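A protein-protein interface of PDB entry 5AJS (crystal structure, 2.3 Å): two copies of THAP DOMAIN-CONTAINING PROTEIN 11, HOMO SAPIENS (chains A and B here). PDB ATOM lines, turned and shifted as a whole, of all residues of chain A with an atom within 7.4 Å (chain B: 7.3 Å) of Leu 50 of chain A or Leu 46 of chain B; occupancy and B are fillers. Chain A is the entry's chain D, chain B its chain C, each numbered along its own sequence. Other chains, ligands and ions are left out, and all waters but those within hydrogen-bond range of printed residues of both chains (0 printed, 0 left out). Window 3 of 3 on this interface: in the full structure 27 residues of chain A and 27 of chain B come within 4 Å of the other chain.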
ATOM      1  N   THR A  42     -10.351   7.212  14.115  1.00  0.00           N
ATOM      2  CA  THR A  42      -9.150   6.860  13.412  1.00  0.00           C
ATOM      3  C   THR A  42      -8.113   7.943  13.355  1.00  0.00           C
ATOM      4  O   THR A  42      -6.915   7.624  13.443  1.00  0.00           O
ATOM      5  CB  THR A  42      -9.465   6.467  11.976  1.00  0.00           C
ATOM      6  OG1 THR A  42     -10.299   5.297  11.997  1.00  0.00           O
ATOM      7  CG2 THR A  42      -8.182   6.139  11.233  1.00  0.00           C
ATOM      8  N   GLU A  43      -8.550   9.200  13.177  1.00  0.00           N
ATOM      9  CA  GLU A  43      -7.626  10.343  13.247  1.00  0.00           C
ATOM     10  C   GLU A  43      -7.032  10.407  14.632  1.00  0.00           C
ATOM     11  O   GLU A  43      -5.801  10.594  14.759  1.00  0.00           O
ATOM     12  CB  GLU A  43      -8.270  11.704  12.904  1.00  0.00           C
ATOM     13  CG  GLU A  43      -7.265  12.867  12.936  1.00  0.00           C
ATOM     14  CD  GLU A  43      -7.749  14.225  12.372  1.00  0.00           C
ATOM     15  OE1 GLU A  43      -8.455  14.311  11.320  1.00  0.00           O
ATOM     16  OE2 GLU A  43      -7.359  15.250  12.985  1.00  0.00           O
ATOM     17  N   ALA A  44      -7.888  10.269  15.665  1.00  0.00           N
ATOM     18  CA  ALA A  44      -7.434  10.447  17.059  1.00  0.00           C
ATOM     19  C   ALA A  44      -6.430   9.369  17.434  1.00  0.00           C
ATOM     20  O   ALA A  44      -5.397   9.644  18.005  1.00  0.00           O
ATOM     21  CB  ALA A  44      -8.622  10.463  18.031  1.00  0.00           C
ATOM     22  N   LYS A  45      -6.715   8.124  17.085  1.00  0.00           N
ATOM     23  CA  LYS A  45      -5.781   7.014  17.304  1.00  0.00           C
ATOM     24  C   LYS A  45      -4.404   7.225  16.660  1.00  0.00           C
ATOM     25  O   LYS A  45      -3.367   6.960  17.267  1.00  0.00           O
ATOM     26  CB  LYS A  45      -6.349   5.715  16.736  1.00  0.00           C
ATOM     27  N   LEU A  46      -4.411   7.680  15.420  1.00  0.00           N
ATOM     28  CA  LEU A  46      -3.194   7.887  14.678  1.00  0.00           C
ATOM     29  C   LEU A  46      -2.415   9.066  15.232  1.00  0.00           C
ATOM     30  O   LEU A  46      -1.177   9.019  15.321  1.00  0.00           O
ATOM     31  CB  LEU A  46      -3.536   8.112  13.208  1.00  0.00           C
ATOM     32  CG  LEU A  46      -4.112   6.881  12.497  1.00  0.00           C
ATOM     33  CD1 LEU A  46      -4.716   7.322  11.191  1.00  0.00           C
ATOM     34  CD2 LEU A  46      -3.058   5.806  12.267  1.00  0.00           C
ATOM     35  N   ARG A  47      -3.116  10.128  15.609  1.00  0.00           N
ATOM     36  CA  ARG A  47      -2.435  11.261  16.217  1.00  0.00           C
ATOM     37  C   ARG A  47      -1.763  10.851  17.511  1.00  0.00           C
ATOM     38  O   ARG A  47      -0.626  11.254  17.786  1.00  0.00           O
ATOM     39  CB  ARG A  47      -3.418  12.396  16.447  1.00  0.00           C
ATOM     40  CG  ARG A  47      -3.812  13.079  15.161  1.00  0.00           C
ATOM     41  CD  ARG A  47      -4.674  14.304  15.399  1.00  0.00           C
ATOM     42  NE  ARG A  47      -5.052  14.899  14.121  1.00  0.00           N
ATOM     43  CZ  ARG A  47      -4.208  15.531  13.299  1.00  0.00           C
ATOM     44  NH1 ARG A  47      -2.914  15.668  13.591  1.00  0.00           N
ATOM     45  NH2 ARG A  47      -4.661  16.035  12.162  1.00  0.00           N
ATOM     46  N   GLU A  48      -2.462  10.031  18.286  1.00  0.00           N
ATOM     47  CA  GLU A  48      -1.960   9.545  19.561  1.00  0.00           C
ATOM     48  C   GLU A  48      -0.719   8.693  19.346  1.00  0.00           C
ATOM     49  O   GLU A  48       0.279   8.784  20.083  1.00  0.00           O
ATOM     50  CB  GLU A  48      -3.026   8.675  20.218  1.00  0.00           C
ATOM     51  N   GLU A  49      -0.787   7.886  18.293  1.00  0.00           N
ATOM     52  CA  GLU A  49       0.222   6.923  18.008  1.00  0.00           C
ATOM     53  C   GLU A  49       1.448   7.622  17.499  1.00  0.00           C
ATOM     54  O   GLU A  49       2.565   7.267  17.862  1.00  0.00           O
ATOM     55  CB  GLU A  49      -0.278   5.858  17.042  1.00  0.00           C
ATOM     56  CG  GLU A  49       0.775   4.759  16.862  1.00  0.00           C
ATOM     57  CD  GLU A  49       0.246   3.465  16.238  1.00  0.00           C
ATOM     58  OE1 GLU A  49      -0.906   3.433  15.719  1.00  0.00           O
ATOM     59  OE2 GLU A  49       0.998   2.461  16.271  1.00  0.00           O
ATOM     60  N   LEU A  50       1.233   8.657  16.717  1.00  0.00           N
ATOM     61  CA  LEU A  50       2.313   9.599  16.379  1.00  0.00           C
ATOM     62  C   LEU A  50       2.947  10.281  17.552  1.00  0.00           C
ATOM     63  O   LEU A  50       4.149  10.575  17.554  1.00  0.00           O
ATOM     64  CB  LEU A  50       1.777  10.731  15.487  1.00  0.00           C
ATOM     65  CG  LEU A  50       1.999  10.293  14.042  1.00  0.00           C
ATOM     66  CD1 LEU A  50       1.062  10.991  13.082  1.00  0.00           C
ATOM     67  CD2 LEU A  50       3.449  10.536  13.651  1.00  0.00           C
ATOM     68  N   ARG A  51       2.095  10.668  18.489  1.00  0.00           N
ATOM     69  CA  ARG A  51       2.519  11.477  19.634  1.00  0.00           C
ATOM     70  C   ARG A  51       3.445  10.621  20.479  1.00  0.00           C
ATOM     71  O   ARG A  51       4.513  11.057  20.888  1.00  0.00           O
ATOM     72  CB  ARG A  51       1.271  11.987  20.367  1.00  0.00           C
ATOM     73  CG  ARG A  51       1.508  12.973  21.483  1.00  0.00           C
ATOM     74  CD  ARG A  51       1.934  14.396  21.110  1.00  0.00           C
ATOM     75  NE  ARG A  51       2.557  15.052  22.277  1.00  0.00           N
ATOM     76  CZ  ARG A  51       2.686  16.365  22.475  1.00  0.00           C
ATOM     77  NH1 ARG A  51       2.222  17.247  21.589  1.00  0.00           N
ATOM     78  NH2 ARG A  51       3.293  16.798  23.584  1.00  0.00           N
ATOM     79  N   GLU A  52       3.117   9.343  20.610  1.00  0.00           N
ATOM     80  CA  GLU A  52       4.027   8.418  21.272  1.00  0.00           C
ATOM     81  C   GLU A  52       5.341   8.146  20.512  1.00  0.00           C
ATOM     82  O   GLU A  52       6.415   8.092  21.100  1.00  0.00           O
ATOM     83  CB  GLU A  52       3.304   7.116  21.559  1.00  0.00           C
ATOM     84  CG  GLU A  52       4.105   6.138  22.407  1.00  0.00           C
ATOM     85  CD  GLU A  52       4.800   6.812  23.611  1.00  0.00           C
ATOM     86  OE1 GLU A  52       4.111   7.492  24.429  1.00  0.00           O
ATOM     87  OE2 GLU A  52       6.044   6.679  23.732  1.00  0.00           O
ATOM     88  N   LYS A  53       5.282   8.000  19.199  1.00  0.00           N
ATOM     89  CA  LYS A  53       6.528   7.776  18.421  1.00  0.00           C
ATOM     90  C   LYS A  53       7.447   8.991  18.323  1.00  0.00           C
ATOM     91  O   LYS A  53       8.657   8.845  18.429  1.00  0.00           O
ATOM     92  CB  LYS A  53       6.194   7.206  17.047  1.00  0.00           C
ATOM     93  CG  LYS A  53       5.350   5.965  17.282  1.00  0.00           C
ATOM     94  CD  LYS A  53       5.444   4.875  16.273  1.00  0.00           C
ATOM     95  CE  LYS A  53       4.653   3.692  16.825  1.00  0.00           C
ATOM     96  NZ  LYS A  53       4.293   2.750  15.736  1.00  0.00           N
ATOM     97  N   ASP A  54       6.903  10.195  18.185  1.00  0.00           N
ATOM     98  CA  ASP A  54       7.747  11.392  18.292  1.00  0.00           C
ATOM     99  C   ASP A  54       8.550  11.417  19.588  1.00  0.00           C
ATOM    100  O   ASP A  54       9.752  11.768  19.594  1.00  0.00           O
ATOM    101  CB  ASP A  54       6.889  12.635  18.300  1.00  0.00           C
ATOM    102  CG  ASP A  54       6.315  12.941  16.946  1.00  0.00           C
ATOM    103  OD1 ASP A  54       6.866  12.440  15.958  1.00  0.00           O
ATOM    104  OD2 ASP A  54       5.321  13.683  16.878  1.00  0.00           O
ATOM    105  N   ARG A  55       7.870  11.063  20.673  1.00  0.00           N
ATOM    106  CA  ARG A  55       8.430  11.159  22.020  1.00  0.00           C
ATOM    107  C   ARG A  55       9.576  10.153  22.174  1.00  0.00           C
ATOM    108  O   ARG A  55      10.676  10.542  22.556  1.00  0.00           O
ATOM    109  CB  ARG A  55       7.311  10.929  23.042  1.00  0.00           C
ATOM    110  CG  ARG A  55       7.678  11.005  24.518  1.00  0.00           C
ATOM    111  CD  ARG A  55       6.425  10.739  25.385  1.00  0.00           C
ATOM    112  NE  ARG A  55       5.358  11.722  25.139  1.00  0.00           N
ATOM    113  CZ  ARG A  55       4.119  11.459  24.683  1.00  0.00           C
ATOM    114  NH1 ARG A  55       3.686  10.215  24.437  1.00  0.00           N
ATOM    115  NH2 ARG A  55       3.270  12.468  24.512  1.00  0.00           N
ATOM    116  N   LEU A  56       9.334   8.888  21.812  1.00  0.00           N
ATOM    117  CA  LEU A  56      10.412   7.846  21.789  1.00  0.00           C
ATOM    118  C   LEU A  56      11.650   8.301  21.020  1.00  0.00           C
ATOM    119  O   LEU A  56      12.755   8.033  21.476  1.00  0.00           O
ATOM    120  CB  LEU A  56       9.937   6.500  21.200  1.00  0.00           C
ATOM    121  CG  LEU A  56       8.885   5.761  22.045  1.00  0.00           C
ATOM    122  CD1 LEU A  56       8.233   4.587  21.315  1.00  0.00           C
ATOM    123  CD2 LEU A  56       9.520   5.277  23.339  1.00  0.00           C
ATOM    124  N   LEU A  57      11.443   8.993  19.887  1.00  0.00           N
ATOM    125  CA  LEU A  57      12.538   9.491  19.040  1.00  0.00           C
ATOM    126  C   LEU A  57      13.234  10.667  19.644  1.00  0.00           C
ATOM    127  O   LEU A  57      14.440  10.799  19.503  1.00  0.00           O
ATOM    128  CB  LEU A  57      12.032   9.958  17.683  1.00  0.00           C
ATOM    129  CG  LEU A  57      11.853   8.833  16.669  1.00  0.00           C
ATOM    130  CD1 LEU A  57      10.977   9.333  15.528  1.00  0.00           C
ATOM    131  CD2 LEU A  57      13.202   8.331  16.167  1.00  0.00           C
ATOM    132  N   LEU B  39     -11.109  14.102   5.727  1.00  0.00           N
ATOM    133  CA  LEU B  39     -10.677  13.110   6.719  1.00  0.00           C
ATOM    134  C   LEU B  39      -9.848  12.011   6.072  1.00  0.00           C
ATOM    135  O   LEU B  39      -8.884  11.525   6.656  1.00  0.00           O
ATOM    136  CB  LEU B  39     -11.869  12.553   7.522  1.00  0.00           C
ATOM    137  CG  LEU B  39     -12.292  13.593   8.610  1.00  0.00           C
ATOM    138  CD1 LEU B  39     -13.670  13.364   9.271  1.00  0.00           C
ATOM    139  CD2 LEU B  39     -11.220  13.713   9.651  1.00  0.00           C
ATOM    140  N   ARG B  40     -10.217  11.597   4.874  1.00  0.00           N
ATOM    141  CA  ARG B  40      -9.485  10.518   4.225  1.00  0.00           C
ATOM    142  C   ARG B  40      -8.025  10.999   3.894  1.00  0.00           C
ATOM    143  O   ARG B  40      -7.040  10.206   3.920  1.00  0.00           O
ATOM    144  CB  ARG B  40     -10.252  10.083   2.982  1.00  0.00           C
ATOM    145  CG  ARG B  40     -11.650   9.495   3.237  1.00  0.00           C
ATOM    146  CD  ARG B  40     -12.515   9.606   1.973  1.00  0.00           C
ATOM    147  NE  ARG B  40     -13.481   8.514   1.739  1.00  0.00           N
ATOM    148  CZ  ARG B  40     -14.400   8.510   0.761  1.00  0.00           C
ATOM    149  NH1 ARG B  40     -14.504   9.536  -0.083  1.00  0.00           N
ATOM    150  NH2 ARG B  40     -15.235   7.483   0.619  1.00  0.00           N
ATOM    151  N   LEU B  41      -7.895  12.303   3.625  1.00  0.00           N
ATOM    152  CA  LEU B  41      -6.608  12.928   3.312  1.00  0.00           C
ATOM    153  C   LEU B  41      -5.827  13.136   4.597  1.00  0.00           C
ATOM    154  O   LEU B  41      -4.623  12.906   4.630  1.00  0.00           O
ATOM    155  CB  LEU B  41      -6.795  14.281   2.630  1.00  0.00           C
ATOM    156  CG  LEU B  41      -6.900  14.227   1.100  1.00  0.00           C
ATOM    157  CD1 LEU B  41      -7.535  15.498   0.517  1.00  0.00           C
ATOM    158  CD2 LEU B  41      -5.519  14.010   0.513  1.00  0.00           C
ATOM    159  N   THR B  42      -6.499  13.573   5.661  1.00  0.00           N
ATOM    160  CA  THR B  42      -5.834  13.570   6.947  1.00  0.00           C
ATOM    161  C   THR B  42      -5.374  12.195   7.416  1.00  0.00           C
ATOM    162  O   THR B  42      -4.253  12.040   7.907  1.00  0.00           O
ATOM    163  CB  THR B  42      -6.690  14.173   8.042  1.00  0.00           C
ATOM    164  OG1 THR B  42      -7.181  15.415   7.578  1.00  0.00           O
ATOM    165  CG2 THR B  42      -5.838  14.416   9.287  1.00  0.00           C
ATOM    166  N   GLU B  43      -6.211  11.189   7.265  1.00  0.00           N
ATOM    167  CA  GLU B  43      -5.758   9.843   7.563  1.00  0.00           C
ATOM    168  C   GLU B  43      -4.504   9.490   6.749  1.00  0.00           C
ATOM    169  O   GLU B  43      -3.531   8.922   7.277  1.00  0.00           O
ATOM    170  CB  GLU B  43      -6.835   8.823   7.236  1.00  0.00           C
ATOM    171  CG  GLU B  43      -6.555   7.424   7.788  1.00  0.00           C
ATOM    172  CD  GLU B  43      -7.638   6.418   7.422  1.00  0.00           C
ATOM    173  OE1 GLU B  43      -8.683   6.846   6.902  1.00  0.00           O
ATOM    174  OE2 GLU B  43      -7.440   5.195   7.657  1.00  0.00           O
ATOM    175  N   ALA B  44      -4.554   9.776   5.451  1.00  0.00           N
ATOM    176  CA  ALA B  44      -3.522   9.302   4.503  1.00  0.00           C
ATOM    177  C   ALA B  44      -2.190   9.924   4.869  1.00  0.00           C
ATOM    178  O   ALA B  44      -1.162   9.235   4.956  1.00  0.00           O
ATOM    179  CB  ALA B  44      -3.901   9.663   3.074  1.00  0.00           C
ATOM    180  N   LYS B  45      -2.223  11.217   5.168  1.00  0.00           N
ATOM    181  CA  LYS B  45      -1.046  11.924   5.632  1.00  0.00           C
ATOM    182  C   LYS B  45      -0.532  11.364   6.949  1.00  0.00           C
ATOM    183  O   LYS B  45       0.684  11.258   7.155  1.00  0.00           O
ATOM    184  CB  LYS B  45      -1.338  13.429   5.803  1.00  0.00           C
ATOM    185  N   LEU B  46      -1.436  11.003   7.849  1.00  0.00           N
ATOM    186  CA  LEU B  46      -1.003  10.502   9.180  1.00  0.00           C
ATOM    187  C   LEU B  46      -0.427   9.072   9.078  1.00  0.00           C
ATOM    188  O   LEU B  46       0.588   8.720   9.669  1.00  0.00           O
ATOM    189  CB  LEU B  46      -2.153  10.578  10.187  1.00  0.00           C
ATOM    190  CG  LEU B  46      -2.506  12.033  10.550  1.00  0.00           C
ATOM    191  CD1 LEU B  46      -3.856  12.133  11.260  1.00  0.00           C
ATOM    192  CD2 LEU B  46      -1.441  12.623  11.429  1.00  0.00           C
ATOM    193  N   ARG B  47      -1.031   8.267   8.240  1.00  0.00           N
ATOM    194  CA  ARG B  47      -0.480   6.957   8.055  1.00  0.00           C
ATOM    195  C   ARG B  47       0.912   7.063   7.395  1.00  0.00           C
ATOM    196  O   ARG B  47       1.817   6.270   7.688  1.00  0.00           O
ATOM    197  CB  ARG B  47      -1.470   6.140   7.285  1.00  0.00           C
ATOM    198  CG  ARG B  47      -2.638   5.626   8.149  1.00  0.00           C
ATOM    199  CD  ARG B  47      -3.483   4.613   7.359  1.00  0.00           C
ATOM    200  NE  ARG B  47      -4.814   4.410   7.922  1.00  0.00           N
ATOM    201  CZ  ARG B  47      -5.079   3.683   9.007  1.00  0.00           C
ATOM    202  NH1 ARG B  47      -4.109   3.053   9.664  1.00  0.00           N
ATOM    203  NH2 ARG B  47      -6.338   3.592   9.440  1.00  0.00           N
ATOM    204  N   GLU B  48       1.115   8.106   6.591  1.00  0.00           N
ATOM    205  CA  GLU B  48       2.413   8.302   5.905  1.00  0.00           C
ATOM    206  C   GLU B  48       3.495   8.645   6.889  1.00  0.00           C
ATOM    207  O   GLU B  48       4.636   8.216   6.744  1.00  0.00           O
ATOM    208  CB  GLU B  48       2.352   9.436   4.874  1.00  0.00           C
ATOM    209  N   GLU B  49       3.107   9.434   7.883  1.00  0.00           N
ATOM    210  CA  GLU B  49       4.008  10.005   8.828  1.00  0.00           C
ATOM    211  C   GLU B  49       4.357   8.898   9.817  1.00  0.00           C
ATOM    212  O   GLU B  49       5.534   8.614  10.116  1.00  0.00           O
ATOM    213  CB  GLU B  49       3.314  11.186   9.487  1.00  0.00           C
ATOM    214  CG  GLU B  49       4.156  11.966  10.487  1.00  0.00           C
ATOM    215  CD  GLU B  49       3.394  13.142  11.109  1.00  0.00           C
ATOM    216  OE1 GLU B  49       2.293  13.477  10.604  1.00  0.00           O
ATOM    217  OE2 GLU B  49       3.885  13.741  12.104  1.00  0.00           O
ATOM    218  N   LEU B  50       3.333   8.253  10.337  1.00  0.00           N
ATOM    219  CA  LEU B  50       3.597   7.100  11.190  1.00  0.00           C
ATOM    220  C   LEU B  50       4.595   6.087  10.625  1.00  0.00           C
ATOM    221  O   LEU B  50       5.483   5.587  11.350  1.00  0.00           O
ATOM    222  CB  LEU B  50       2.288   6.382  11.481  1.00  0.00           C
ATOM    223  CG  LEU B  50       1.505   6.931  12.663  1.00  0.00           C
ATOM    224  CD1 LEU B  50       0.084   6.426  12.550  1.00  0.00           C
ATOM    225  CD2 LEU B  50       2.128   6.492  13.988  1.00  0.00           C
ATOM    226  N   ARG B  51       4.417   5.733   9.360  1.00  0.00           N
ATOM    227  CA  ARG B  51       5.310   4.758   8.661  1.00  0.00           C
ATOM    228  C   ARG B  51       6.760   5.279   8.557  1.00  0.00           C
ATOM    229  O   ARG B  51       7.697   4.531   8.699  1.00  0.00           O
ATOM    230  CB  ARG B  51       4.753   4.495   7.243  1.00  0.00           C
ATOM    231  CG  ARG B  51       5.382   3.329   6.493  1.00  0.00           C
ATOM    232  CD  ARG B  51       4.990   1.943   7.014  1.00  0.00           C
ATOM    233  NE  ARG B  51       5.899   0.972   6.402  1.00  0.00           N
ATOM    234  CZ  ARG B  51       5.742   0.410   5.199  1.00  0.00           C
ATOM    235  NH1 ARG B  51       4.668   0.649   4.447  1.00  0.00           N
ATOM    236  NH2 ARG B  51       6.660  -0.433   4.750  1.00  0.00           N
ATOM    237  N   GLU B  52       6.935   6.580   8.338  1.00  0.00           N
ATOM    238  CA  GLU B  52       8.233   7.209   8.473  1.00  0.00           C
ATOM    239  C   GLU B  52       8.772   7.197   9.872  1.00  0.00           C
ATOM    240  O   GLU B  52       9.987   7.123  10.062  1.00  0.00           O
ATOM    241  CB  GLU B  52       8.197   8.668   7.983  1.00  0.00           C
ATOM    242  CG  GLU B  52       9.572   9.335   7.998  1.00  0.00           C
ATOM    243  CD  GLU B  52      10.677   8.449   7.332  1.00  0.00           C
ATOM    244  OE1 GLU B  52      10.422   7.761   6.290  1.00  0.00           O
ATOM    245  OE2 GLU B  52      11.815   8.425   7.844  1.00  0.00           O
ATOM    246  N   LYS B  53       7.929   7.270  10.885  1.00  0.00           N
ATOM    247  CA  LYS B  53       8.529   7.258  12.252  1.00  0.00           C
ATOM    248  C   LYS B  53       8.875   5.900  12.725  1.00  0.00           C
ATOM    249  O   LYS B  53       9.860   5.719  13.470  1.00  0.00           O
ATOM    250  CB  LYS B  53       7.677   8.000  13.266  1.00  0.00           C
ATOM    251  CG  LYS B  53       7.490   9.422  12.748  1.00  0.00           C
ATOM    252  CD  LYS B  53       7.203  10.485  13.782  1.00  0.00           C
ATOM    253  CE  LYS B  53       7.673  11.834  13.246  1.00  0.00           C
ATOM    254  NZ  LYS B  53       6.812  12.977  13.647  1.00  0.00           N
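The side-chain carboxylate (OD2) of Asp 54 of chain A lies within salt-bridge range of the side-chain amino group (NZ) of Lys 53 of chain B (3.6 Å).
Of the 15 printed residues of chain B, 8 touch a printed residue of chain A. Hydrophobic or aromatic side chains of chain B within 4 Å of the printed part of chain A: Leu 39, Leu 46 and Leu 50. Of the 16 printed residues of chain A, 7 touch a printed residue of chain B. Hydrophobic or aromatic side chains of chain A within 4 Å of the printed part of chain B: Leu 46 and Leu 50. Among the printed residues, Asp or Glu carboxylates within 4 Å of a Lys or Arg side-chain nitrogen of the other chain: Asp 54 of chain A with Lys 53 of chain B (2.4 Å).
Thr 42 of chain A touches Glu 43 of chain B, and with the chains exchanged Glu 43 of chain A touches Thr 42 of chain B. Glu 43 of chain A touches Leu 46 of chain B, and with the chains exchanged Leu 46 of chain A touches Glu 43 of chain B. Glu 49 of chain A touches Leu 50 of chain B, and with the chains exchanged Leu 50 of chain A touches Glu 49 of chain B. Leu 50 of chain A touches Lys 53 of chain B, but with the chains exchanged Lys 53 of chain A does not touch Leu 50 of chain B (4.3 Å). Of the 16 pairs that touch across the chains among the printed residues, 13 have their exchanged pair printed and touching as well.
Of chain B, only Leu 46 (3.4 Å), Glu 49 (3.5 Å), Leu 50 (3.6 Å) and Lys 53 (3.8 Å) come within 4 Å of Leu 50 of chain A. Of the printed residues of chain A, Leu 46 of chain B touches Glu 43 (3.9 Å), Arg 47 (3.98 Å) and Leu 50 (3.4 Å). Lys 45 of chain B touches none of the printed residues of chain A. Printed residues of chain A within 4 Å of Glu 43 of chain B: Thr 42 and Leu 46. Printed residues of chain B within 4 Å of Glu 49 of chain A: Leu 50 (3.6 Å). Printed residues of chain A within 4 Å of Arg 47 of chain B: Thr 42 (3.6 Å) and Leu 46 (3.9 Å). Of the printed residues of chain B, Thr 42 of chain A touches Glu 43 and Arg 47. Arg 55 of chain A touches none of the printed residues of chain B. Arg 51 of chain A touches none of the printed residues of chain B.
Glu 43 of chain B touches Thr 42 of chain A (OE2 to CG2, 3.8 Å). OE1 of Glu 43 of chain A touches CD2 of Leu 39 of chain B, 3.3 Å away. OE1 of Glu 43 of chain A touches CG2 of Thr 42 of chain B (3.3 Å). CD1 of Leu 46 of chain B touches CG of Glu 43 of chain A, 3.9 Å away. Leu 46 of chain A touches Arg 47 of chain B. Thr 42 of chain B touches Arg 47 of chain A. Arg 47 of chain A touches Leu 46 of chain B. CG of Glu 49 of chain A touches CD2 of Leu 50 of chain B, at 3.6 Å. Leu 50 of chain A touches Leu 50 of chain B. Lys 53 of chain B touches Leu 50 of chain A.
The side-chain amino group of Lys 53 of chain A is in salt-bridge range of the side-chain carboxylate of Glu 49 of chain A (3.4 Å). OE2 of Glu 49 of chain B is in salt-bridge range of NZ of Lys 53 of chain B, 3.4 Å away. NH2 of Arg 47 of chain B lies within salt-bridge range of OE2 of Glu 43 of chain B (2.6 Å). The side-chain carboxylate (OE2) of Glu 43 of chain A lies within salt-bridge range of the guanidinium group (NE) of Arg 47 of chain A (2.6 Å).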
